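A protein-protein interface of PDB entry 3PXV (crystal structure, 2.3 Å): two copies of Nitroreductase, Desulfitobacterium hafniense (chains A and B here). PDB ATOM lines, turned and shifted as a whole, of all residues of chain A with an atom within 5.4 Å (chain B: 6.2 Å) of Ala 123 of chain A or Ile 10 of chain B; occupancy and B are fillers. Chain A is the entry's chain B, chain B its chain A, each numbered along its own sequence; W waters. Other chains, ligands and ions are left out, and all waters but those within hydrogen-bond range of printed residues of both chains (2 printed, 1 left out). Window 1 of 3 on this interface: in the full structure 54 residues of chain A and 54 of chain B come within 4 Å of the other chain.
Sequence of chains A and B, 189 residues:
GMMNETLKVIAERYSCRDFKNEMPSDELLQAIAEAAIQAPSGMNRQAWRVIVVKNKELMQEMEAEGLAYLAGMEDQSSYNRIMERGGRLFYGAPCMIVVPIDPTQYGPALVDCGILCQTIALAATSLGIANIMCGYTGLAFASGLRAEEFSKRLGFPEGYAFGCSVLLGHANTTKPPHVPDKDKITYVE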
ATOM      1  N   ALA A  31      19.196 -26.300 -11.096  1.00  0.00           N
ATOM      2  CA  ALA A  31      19.280 -27.147  -9.896  1.00  0.00           C
ATOM      3  C   ALA A  31      19.265 -26.287  -8.650  1.00  0.00           C
ATOM      4  O   ALA A  31      18.608 -26.631  -7.665  1.00  0.00           O
ATOM      5  CB  ALA A  31      20.540 -28.003  -9.914  1.00  0.00           C
ATOM      6  N   ILE A  32      19.980 -25.159  -8.713  1.00  0.00           N
ATOM      7  CA  ILE A  32      20.057 -24.216  -7.610  1.00  0.00           C
ATOM      8  C   ILE A  32      18.715 -23.504  -7.361  1.00  0.00           C
ATOM      9  O   ILE A  32      18.298 -23.331  -6.202  1.00  0.00           O
ATOM     10  CB  ILE A  32      21.141 -23.167  -7.880  1.00  0.00           C
ATOM     11  CG1 ILE A  32      22.529 -23.831  -7.867  1.00  0.00           C
ATOM     12  CG2 ILE A  32      21.040 -22.015  -6.859  1.00  0.00           C
ATOM     13  CD1 ILE A  32      23.659 -22.924  -8.429  1.00  0.00           C
ATOM     14  N   ALA A  35      16.280 -25.898  -5.841  1.00  0.00           N
ATOM     15  CA  ALA A  35      16.601 -26.100  -4.438  1.00  0.00           C
ATOM     16  C   ALA A  35      16.017 -24.949  -3.616  1.00  0.00           C
ATOM     17  O   ALA A  35      15.429 -25.164  -2.559  1.00  0.00           O
ATOM     18  CB  ALA A  35      18.112 -26.205  -4.251  1.00  0.00           C
ATOM     19  N   ALA A  36      16.134 -23.730  -4.126  1.00  0.00           N
ATOM     20  CA  ALA A  36      15.624 -22.560  -3.414  1.00  0.00           C
ATOM     21  C   ALA A  36      14.119 -22.665  -3.120  1.00  0.00           C
ATOM     22  O   ALA A  36      13.675 -22.443  -2.000  1.00  0.00           O
ATOM     23  CB  ALA A  36      15.941 -21.277  -4.203  1.00  0.00           C
ATOM     24  N   GLN A  38      12.453 -25.138  -2.616  1.00  0.00           N
ATOM     25  CA  GLN A  38      12.198 -26.221  -1.660  1.00  0.00           C
ATOM     26  C   GLN A  38      12.435 -25.725  -0.222  1.00  0.00           C
ATOM     27  O   GLN A  38      12.284 -26.479   0.756  1.00  0.00           O
ATOM     28  CB  GLN A  38      13.058 -27.457  -1.983  1.00  0.00           C
ATOM     29  CG  GLN A  38      12.698 -28.130  -3.314  1.00  0.00           C
ATOM     30  CD  GLN A  38      13.770 -29.071  -3.874  1.00  0.00           C
ATOM     31  OE1 GLN A  38      14.961 -28.970  -3.558  1.00  0.00           O
ATOM     32  NE2 GLN A  38      13.341 -29.972  -4.759  1.00  0.00           N
ATOM     33  N   ALA A  39      12.790 -24.448  -0.102  1.00  0.00           N
ATOM     34  CA  ALA A  39      12.988 -23.835   1.203  1.00  0.00           C
ATOM     35  C   ALA A  39      11.665 -23.776   1.968  1.00  0.00           C
ATOM     36  O   ALA A  39      10.618 -23.515   1.388  1.00  0.00           O
ATOM     37  CB  ALA A  39      13.567 -22.410   1.043  1.00  0.00           C
ATOM     38  N   GLN A 118      20.150 -19.140   2.178  1.00  0.00           N
ATOM     39  CA  GLN A 118      21.085 -20.181   2.653  1.00  0.00           C
ATOM     40  C   GLN A 118      20.873 -21.450   1.829  1.00  0.00           C
ATOM     41  O   GLN A 118      21.833 -22.113   1.459  1.00  0.00           O
ATOM     42  CB  GLN A 118      20.939 -20.446   4.162  1.00  0.00           C
ATOM     43  CG  GLN A 118      21.827 -21.536   4.736  1.00  0.00           C
ATOM     44  CD  GLN A 118      23.327 -21.270   4.647  1.00  0.00           C
ATOM     45  OE1 GLN A 118      23.764 -20.412   3.918  1.00  0.00           O
ATOM     46  NE2 GLN A 118      24.119 -22.035   5.389  1.00  0.00           N
ATOM     47  N   THR A 119      19.630 -21.785   1.510  1.00  0.00           N
ATOM     48  CA  THR A 119      19.388 -22.973   0.688  1.00  0.00           C
ATOM     49  C   THR A 119      20.092 -22.827  -0.671  1.00  0.00           C
ATOM     50  O   THR A 119      20.726 -23.770  -1.169  1.00  0.00           O
ATOM     51  CB  THR A 119      17.928 -23.203   0.495  1.00  0.00           C
ATOM     52  OG1 THR A 119      17.308 -23.298   1.779  1.00  0.00           O
ATOM     53  CG2 THR A 119      17.692 -24.486  -0.308  1.00  0.00           C
ATOM     54  N   ILE A 120      20.020 -21.629  -1.250  1.00  0.00           N
ATOM     55  CA  ILE A 120      20.736 -21.347  -2.487  1.00  0.00           C
ATOM     56  C   ILE A 120      22.251 -21.547  -2.292  1.00  0.00           C
ATOM     57  O   ILE A 120      22.898 -22.273  -3.062  1.00  0.00           O
ATOM     58  CB  ILE A 120      20.510 -19.884  -2.984  1.00  0.00           C
ATOM     59  CG1 ILE A 120      19.046 -19.676  -3.375  1.00  0.00           C
ATOM     60  CG2 ILE A 120      21.475 -19.578  -4.143  1.00  0.00           C
ATOM     61  CD1 ILE A 120      18.681 -18.286  -3.851  1.00  0.00           C
ATOM     62  N   ALA A 121      22.806 -20.910  -1.259  1.00  0.00           N
ATOM     63  CA  ALA A 121      24.250 -20.939  -1.056  1.00  0.00           C
ATOM     64  C   ALA A 121      24.744 -22.362  -0.869  1.00  0.00           C
ATOM     65  O   ALA A 121      25.762 -22.752  -1.458  1.00  0.00           O
ATOM     66  CB  ALA A 121      24.673 -20.032   0.129  1.00  0.00           C
ATOM     67  N   LEU A 122      24.023 -23.150  -0.075  1.00  0.00           N
ATOM     68  CA  LEU A 122      24.434 -24.538   0.149  1.00  0.00           C
ATOM     69  C   LEU A 122      24.291 -25.356  -1.130  1.00  0.00           C
ATOM     70  O   LEU A 122      25.184 -26.149  -1.481  1.00  0.00           O
ATOM     71  CB  LEU A 122      23.689 -25.183   1.340  1.00  0.00           C
ATOM     72  CG  LEU A 122      23.987 -24.533   2.694  1.00  0.00           C
ATOM     73  CD1 LEU A 122      23.275 -25.262   3.806  1.00  0.00           C
ATOM     74  CD2 LEU A 122      25.483 -24.481   2.994  1.00  0.00           C
ATOM     75  N   ALA A 123      23.187 -25.161  -1.851  1.00  0.00           N
ATOM     76  CA  ALA A 123      23.016 -25.887  -3.125  1.00  0.00           C
ATOM     77  C   ALA A 123      24.142 -25.534  -4.112  1.00  0.00           C
ATOM     78  O   ALA A 123      24.714 -26.402  -4.747  1.00  0.00           O
ATOM     79  CB  ALA A 123      21.633 -25.634  -3.729  1.00  0.00           C
ATOM     80  N   ALA A 124      24.482 -24.258  -4.209  1.00  0.00           N
ATOM     81  CA  ALA A 124      25.530 -23.831  -5.130  1.00  0.00           C
ATOM     82  C   ALA A 124      26.870 -24.445  -4.732  1.00  0.00           C
ATOM     83  O   ALA A 124      27.637 -24.951  -5.577  1.00  0.00           O
ATOM     84  CB  ALA A 124      25.622 -22.319  -5.150  1.00  0.00           C
ATOM     85  N   THR A 125      27.140 -24.444  -3.432  1.00  0.00           N
ATOM     86  CA  THR A 125      28.423 -24.928  -2.933  1.00  0.00           C
ATOM     87  C   THR A 125      28.578 -26.418  -3.206  1.00  0.00           C
ATOM     88  O   THR A 125      29.676 -26.849  -3.533  1.00  0.00           O
ATOM     89  CB  THR A 125      28.614 -24.619  -1.440  1.00  0.00           C
ATOM     90  OG1 THR A 125      28.600 -23.200  -1.239  1.00  0.00           O
ATOM     91  CG2 THR A 125      29.907 -25.153  -0.968  1.00  0.00           C
ATOM     92  N   SER A 126      27.486 -27.181  -3.073  1.00  0.00           N
ATOM     93  CA  SER A 126      27.499 -28.630  -3.335  1.00  0.00           C
ATOM     94  C   SER A 126      27.751 -28.912  -4.797  1.00  0.00           C
ATOM     95  O   SER A 126      28.201 -30.006  -5.143  1.00  0.00           O
ATOM     96  CB  SER A 126      26.156 -29.282  -2.996  1.00  0.00           C
ATOM     97  OG  SER A 126      25.172 -28.963  -3.972  1.00  0.00           O
ATOM     98  N   LEU A 127      27.400 -27.946  -5.652  1.00  0.00           N
ATOM     99  CA  LEU A 127      27.577 -28.076  -7.116  1.00  0.00           C
ATOM    100  C   LEU A 127      28.878 -27.491  -7.626  1.00  0.00           C
ATOM    101  O   LEU A 127      29.098 -27.437  -8.822  1.00  0.00           O
ATOM    102  CB  LEU A 127      26.389 -27.448  -7.864  1.00  0.00           C
ATOM    103  CG  LEU A 127      25.068 -28.199  -7.689  1.00  0.00           C
ATOM    104  CD1 LEU A 127      23.868 -27.432  -8.262  1.00  0.00           C
ATOM    105  CD2 LEU A 127      25.211 -29.552  -8.342  1.00  0.00           C
ATOM    106  N   ASN B   4      22.726 -34.656  -6.043  1.00  0.00           N
ATOM    107  CA  ASN B   4      23.833 -35.026  -5.148  1.00  0.00           C
ATOM    108  C   ASN B   4      23.194 -35.162  -3.752  1.00  0.00           C
ATOM    109  O   ASN B   4      22.011 -34.874  -3.618  1.00  0.00           O
ATOM    110  CB  ASN B   4      24.998 -34.009  -5.201  1.00  0.00           C
ATOM    111  CG  ASN B   4      24.627 -32.621  -4.673  1.00  0.00           C
ATOM    112  OD1 ASN B   4      23.867 -32.484  -3.717  1.00  0.00           O
ATOM    113  ND2 ASN B   4      25.219 -31.579  -5.268  1.00  0.00           N
ATOM    114  N   GLU B   5      23.928 -35.589  -2.727  1.00  0.00           N
ATOM    115  CA  GLU B   5      23.321 -35.756  -1.385  1.00  0.00           C
ATOM    116  C   GLU B   5      22.758 -34.446  -0.795  1.00  0.00           C
ATOM    117  O   GLU B   5      21.728 -34.466  -0.127  1.00  0.00           O
ATOM    118  CB  GLU B   5      24.290 -36.395  -0.369  1.00  0.00           C
ATOM    119  CG  GLU B   5      24.590 -37.902  -0.578  1.00  0.00           C
ATOM    120  CD  GLU B   5      25.534 -38.524   0.482  1.00  0.00           C
ATOM    121  OE1 GLU B   5      25.680 -37.992   1.621  1.00  0.00           O
ATOM    122  OE2 GLU B   5      26.130 -39.570   0.165  1.00  0.00           O
ATOM    123  N   THR B   6      23.426 -33.315  -1.023  1.00  0.00           N
ATOM    124  CA  THR B   6      22.940 -32.055  -0.445  1.00  0.00           C
ATOM    125  C   THR B   6      21.639 -31.637  -1.119  1.00  0.00           C
ATOM    126  O   THR B   6      20.699 -31.210  -0.453  1.00  0.00           O
ATOM    127  CB  THR B   6      23.987 -30.947  -0.540  1.00  0.00           C
ATOM    128  OG1 THR B   6      25.134 -31.351   0.204  1.00  0.00           O
ATOM    129  CG2 THR B   6      23.456 -29.625   0.004  1.00  0.00           C
ATOM    130  N   LEU B   7      21.561 -31.812  -2.432  1.00  0.00           N
ATOM    131  CA  LEU B   7      20.350 -31.459  -3.112  1.00  0.00           C
ATOM    132  C   LEU B   7      19.207 -32.384  -2.681  1.00  0.00           C
ATOM    133  O   LEU B   7      18.078 -31.914  -2.585  1.00  0.00           O
ATOM    134  CB  LEU B   7      20.545 -31.423  -4.628  1.00  0.00           C
ATOM    135  CG  LEU B   7      21.491 -30.355  -5.194  1.00  0.00           C
ATOM    136  CD1 LEU B   7      21.763 -30.655  -6.675  1.00  0.00           C
ATOM    137  CD2 LEU B   7      20.955 -28.951  -4.977  1.00  0.00           C
ATOM    138  N   LYS B   8      19.485 -33.657  -2.385  1.00  0.00           N
ATOM    139  CA  LYS B   8      18.422 -34.572  -1.954  1.00  0.00           C
ATOM    140  C   LYS B   8      17.943 -34.204  -0.556  1.00  0.00           C
ATOM    141  O   LYS B   8      16.770 -34.302  -0.282  1.00  0.00           O
ATOM    142  CB  LYS B   8      18.815 -36.078  -2.020  1.00  0.00           C
ATOM    143  N   VAL B   9      18.846 -33.794   0.324  1.00  0.00           N
ATOM    144  CA  VAL B   9      18.470 -33.404   1.675  1.00  0.00           C
ATOM    145  C   VAL B   9      17.541 -32.190   1.601  1.00  0.00           C
ATOM    146  O   VAL B   9      16.518 -32.173   2.231  1.00  0.00           O
ATOM    147  CB  VAL B   9      19.720 -33.151   2.595  1.00  0.00           C
ATOM    148  CG1 VAL B   9      19.348 -32.374   3.839  1.00  0.00           C
ATOM    149  CG2 VAL B   9      20.423 -34.462   2.965  1.00  0.00           C
ATOM    150  N   ILE B  10      17.895 -31.198   0.789  1.00  0.00           N
ATOM    151  CA  ILE B  10      17.106 -29.986   0.651  1.00  0.00           C
ATOM    152  C   ILE B  10      15.690 -30.337   0.180  1.00  0.00           C
ATOM    153  O   ILE B  10      14.708 -29.800   0.712  1.00  0.00           O
ATOM    154  CB  ILE B  10      17.813 -28.996  -0.327  1.00  0.00           C
ATOM    155  CG1 ILE B  10      19.116 -28.459   0.296  1.00  0.00           C
ATOM    156  CG2 ILE B  10      16.892 -27.841  -0.748  1.00  0.00           C
ATOM    157  CD1 ILE B  10      20.082 -27.727  -0.716  1.00  0.00           C
ATOM    158  N   ALA B  11      15.589 -31.269  -0.783  1.00  0.00           N
ATOM    159  CA  ALA B  11      14.298 -31.700  -1.350  1.00  0.00           C
ATOM    160  C   ALA B  11      13.446 -32.601  -0.433  1.00  0.00           C
ATOM    161  O   ALA B  11      12.196 -32.582  -0.524  1.00  0.00           O
ATOM    162  CB  ALA B  11      14.493 -32.409  -2.738  1.00  0.00           C
ATOM    163  N   GLU B  12      14.101 -33.397   0.410  1.00  0.00           N
ATOM    164  CA  GLU B  12      13.378 -34.329   1.272  1.00  0.00           C
ATOM    165  C   GLU B  12      13.101 -33.762   2.698  1.00  0.00           C
ATOM    166  O   GLU B  12      12.278 -34.278   3.428  1.00  0.00           O
ATOM    167  CB  GLU B  12      14.086 -35.706   1.285  1.00  0.00           C
ATOM    168  CG  GLU B  12      15.322 -35.807   2.186  1.00  0.00           C
ATOM    169  CD  GLU B  12      16.132 -37.113   1.998  1.00  0.00           C
ATOM    170  OE1 GLU B  12      15.745 -37.965   1.134  1.00  0.00           O
ATOM    171  OE2 GLU B  12      17.159 -37.266   2.730  1.00  0.00           O
ATOM    172  N   ARG B  13      13.785 -32.701   3.090  1.00  0.00           N
ATOM    173  CA  ARG B  13      13.503 -32.109   4.398  1.00  0.00           C
ATOM    174  C   ARG B  13      11.996 -31.760   4.437  1.00  0.00           C
ATOM    175  O   ARG B  13      11.446 -31.267   3.454  1.00  0.00           O
ATOM    176  CB  ARG B  13      14.341 -30.843   4.626  1.00  0.00           C
ATOM    177  CG  ARG B  13      14.039 -30.060   5.941  1.00  0.00           C
ATOM    178  CD  ARG B  13      14.052 -28.552   5.685  1.00  0.00           C
ATOM    179  NE  ARG B  13      13.175 -28.272   4.532  1.00  0.00           N
ATOM    180  CZ  ARG B  13      11.847 -28.201   4.583  1.00  0.00           C
ATOM    181  NH1 ARG B  13      11.203 -28.352   5.726  1.00  0.00           N
ATOM    182  NH2 ARG B  13      11.152 -27.965   3.479  1.00  0.00           N
ATOM    183  N   GLN B 118      17.820 -22.716   8.892  1.00  0.00           N
ATOM    184  CA  GLN B 118      17.764 -23.631   7.751  1.00  0.00           C
ATOM    185  C   GLN B 118      19.004 -24.497   7.774  1.00  0.00           C
ATOM    186  O   GLN B 118      18.928 -25.628   7.339  1.00  0.00           O
ATOM    187  CB  GLN B 118      17.597 -22.905   6.407  1.00  0.00           C
ATOM    188  CG  GLN B 118      17.696 -23.786   5.126  1.00  0.00           C
ATOM    189  CD  GLN B 118      16.527 -24.744   4.902  1.00  0.00           C
ATOM    190  OE1 GLN B 118      15.803 -25.068   5.822  1.00  0.00           O
ATOM    191  NE2 GLN B 118      16.369 -25.223   3.666  1.00  0.00           N
ATOM    192  N   LEU B 122      18.675 -28.582   7.641  1.00  0.00           N
ATOM    193  CA  LEU B 122      19.341 -29.408   6.631  1.00  0.00           C
ATOM    194  C   LEU B 122      20.386 -30.360   7.285  1.00  0.00           C
ATOM    195  O   LEU B 122      20.426 -31.553   6.964  1.00  0.00           O
ATOM    196  CB  LEU B 122      19.930 -28.521   5.542  1.00  0.00           C
ATOM    197  CG  LEU B 122      18.857 -27.698   4.799  1.00  0.00           C
ATOM    198  CD1 LEU B 122      19.539 -26.714   3.845  1.00  0.00           C
ATOM    199  CD2 LEU B 122      17.832 -28.576   4.026  1.00  0.00           C
ATOM    200  N   THR B 125      18.296 -33.097   9.053  1.00  0.00           N
ATOM    201  CA  THR B 125      17.738 -34.007   8.034  1.00  0.00           C
ATOM    202  C   THR B 125      18.794 -34.958   7.452  1.00  0.00           C
ATOM    203  O   THR B 125      18.551 -36.144   7.265  1.00  0.00           O
ATOM    204  CB  THR B 125      17.086 -33.206   6.875  1.00  0.00           C
ATOM    205  OG1 THR B 125      16.015 -32.405   7.396  1.00  0.00           O
ATOM    206  CG2 THR B 125      16.538 -34.146   5.745  1.00  0.00           C
HETATM  207  O   HOH W   1      17.290 -29.949  -4.443  1.00  0.00           O
HETATM  208  O   HOH W   2      14.473 -27.549   2.020  1.00  0.00           O
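OG of Ser 126 of chain A lies within hydrogen-bond range of ND2 of Asn 4 of chain B (2.9 Å).
NH2 of Arg 13 of chain B sits at hydrogen-bond distance from O of Gln 38 of chain A, at 3.3 Å.
NE2 of Gln 118 of chain B is in hydrogen-bond range of OG1 of Thr 119 of chain A (2.9 Å).
Of the 16 printed residues of chain A, 6 touch a printed residue of chain B.
Hydrophobic or aromatic side chains of chain A within 4 Å of the printed part of chain B: Ala 123 and Leu 127.
Of the 13 printed residues of chain B, 7 touch a printed residue of chain A.
Hydrophobic or aromatic side chains of chain B that line the printed part of chain A: Leu 7, Ile 10 and Ala 11.
Among the printed residues, no Asp or Glu carboxylate lies within 4 Å of a Lys or Arg side-chain nitrogen of the other chain.
N of Thr 6 of chain B lies within hydrogen-bond range of OD1 of Asn 4 of chain B, at 2.9 Å.
The side-chain amide oxygen (OD1) of Asn 4 of chain B sits at hydrogen-bond distance from the backbone NH (N) of Leu 7 of chain B, 2.7 Å away.
The side-chain hydroxyl of Ser 126 of chain A lies within hydrogen-bond range of the backbone carbonyl oxygen of Ala 123 of chain A, 2.7 Å away.
Among the printed residues, merely in contact across the chains: Gln 38 of chain A with Ala 11 of chain B (3.4 Å), Thr 119 of chain A with Ile 10 of chain B (3.5 Å), Ala 35 of chain A with Ile 10 of chain B (3.5 Å), Gln 38 of chain A with Ile 10 of chain B (3.6 Å), Ala 123 of chain A with Leu 7 of chain B (3.6 Å), Ser 126 of chain A with Thr 6 of chain B (3.7 Å), Leu 127 of chain A with Asn 4 of chain B (3.7 Å), Ala 123 of chain A with Ile 10 of chain B (3.98 Å) and Leu 127 of chain A with Leu 7 of chain B (3.99 Å).
3 positions are printed for both chains.
Water W2 lies within hydrogen-bond range of O of Ile 10 of chain B (2.6 Å), O of Gln 38 of chain A (2.7 Å), NE of Arg 13 of chain B (2.9 Å) and NE2 of Gln 118 of chain B (3.4 Å).
Water W1 bridges OE1 of Gln 38 of chain A and O of Leu 7 of chain B.
Printed residues of chain B within 4 Å of Ala 123 of chain A: Leu 7 and Ile 10.
Of the printed residues of chain A, Ile 10 of chain B touches Ala 35 (3.5 Å), Gln 38 (3.6 Å), Thr 119 (3.5 Å) and Ala 123 (3.98 Å).
Printed residues of chain A within 4 Å of Asn 4 of chain B: Ser 126 and Leu 127.
Of the printed residues of chain A, Thr 6 of chain B touches Ser 126 (3.7 Å).
Printed residues of chain B within 4 Å of Thr 119 of chain A: Ile 10 (3.5 Å) and Gln 118 (2.9 Å).
Printed residues of chain B within 4 Å of Gln 38 of chain A: Ile 10 (3.6 Å), Ala 11 (3.4 Å) and Arg 13 (3.3 Å).
Ala 121 of chain A touches none of the printed residues of chain B.
The nearest printed residue of chain B that does not touch Ala 123 of chain A is Thr 6 of chain B (4.8 Å).
The nearest printed residue of chain A that does not touch Ile 10 of chain B is Leu 122 of chain A (4.8 Å).
The nearest printed residue of chain B that does not touch Gln 38 of chain A is Leu 7 of chain B (4.4 Å).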
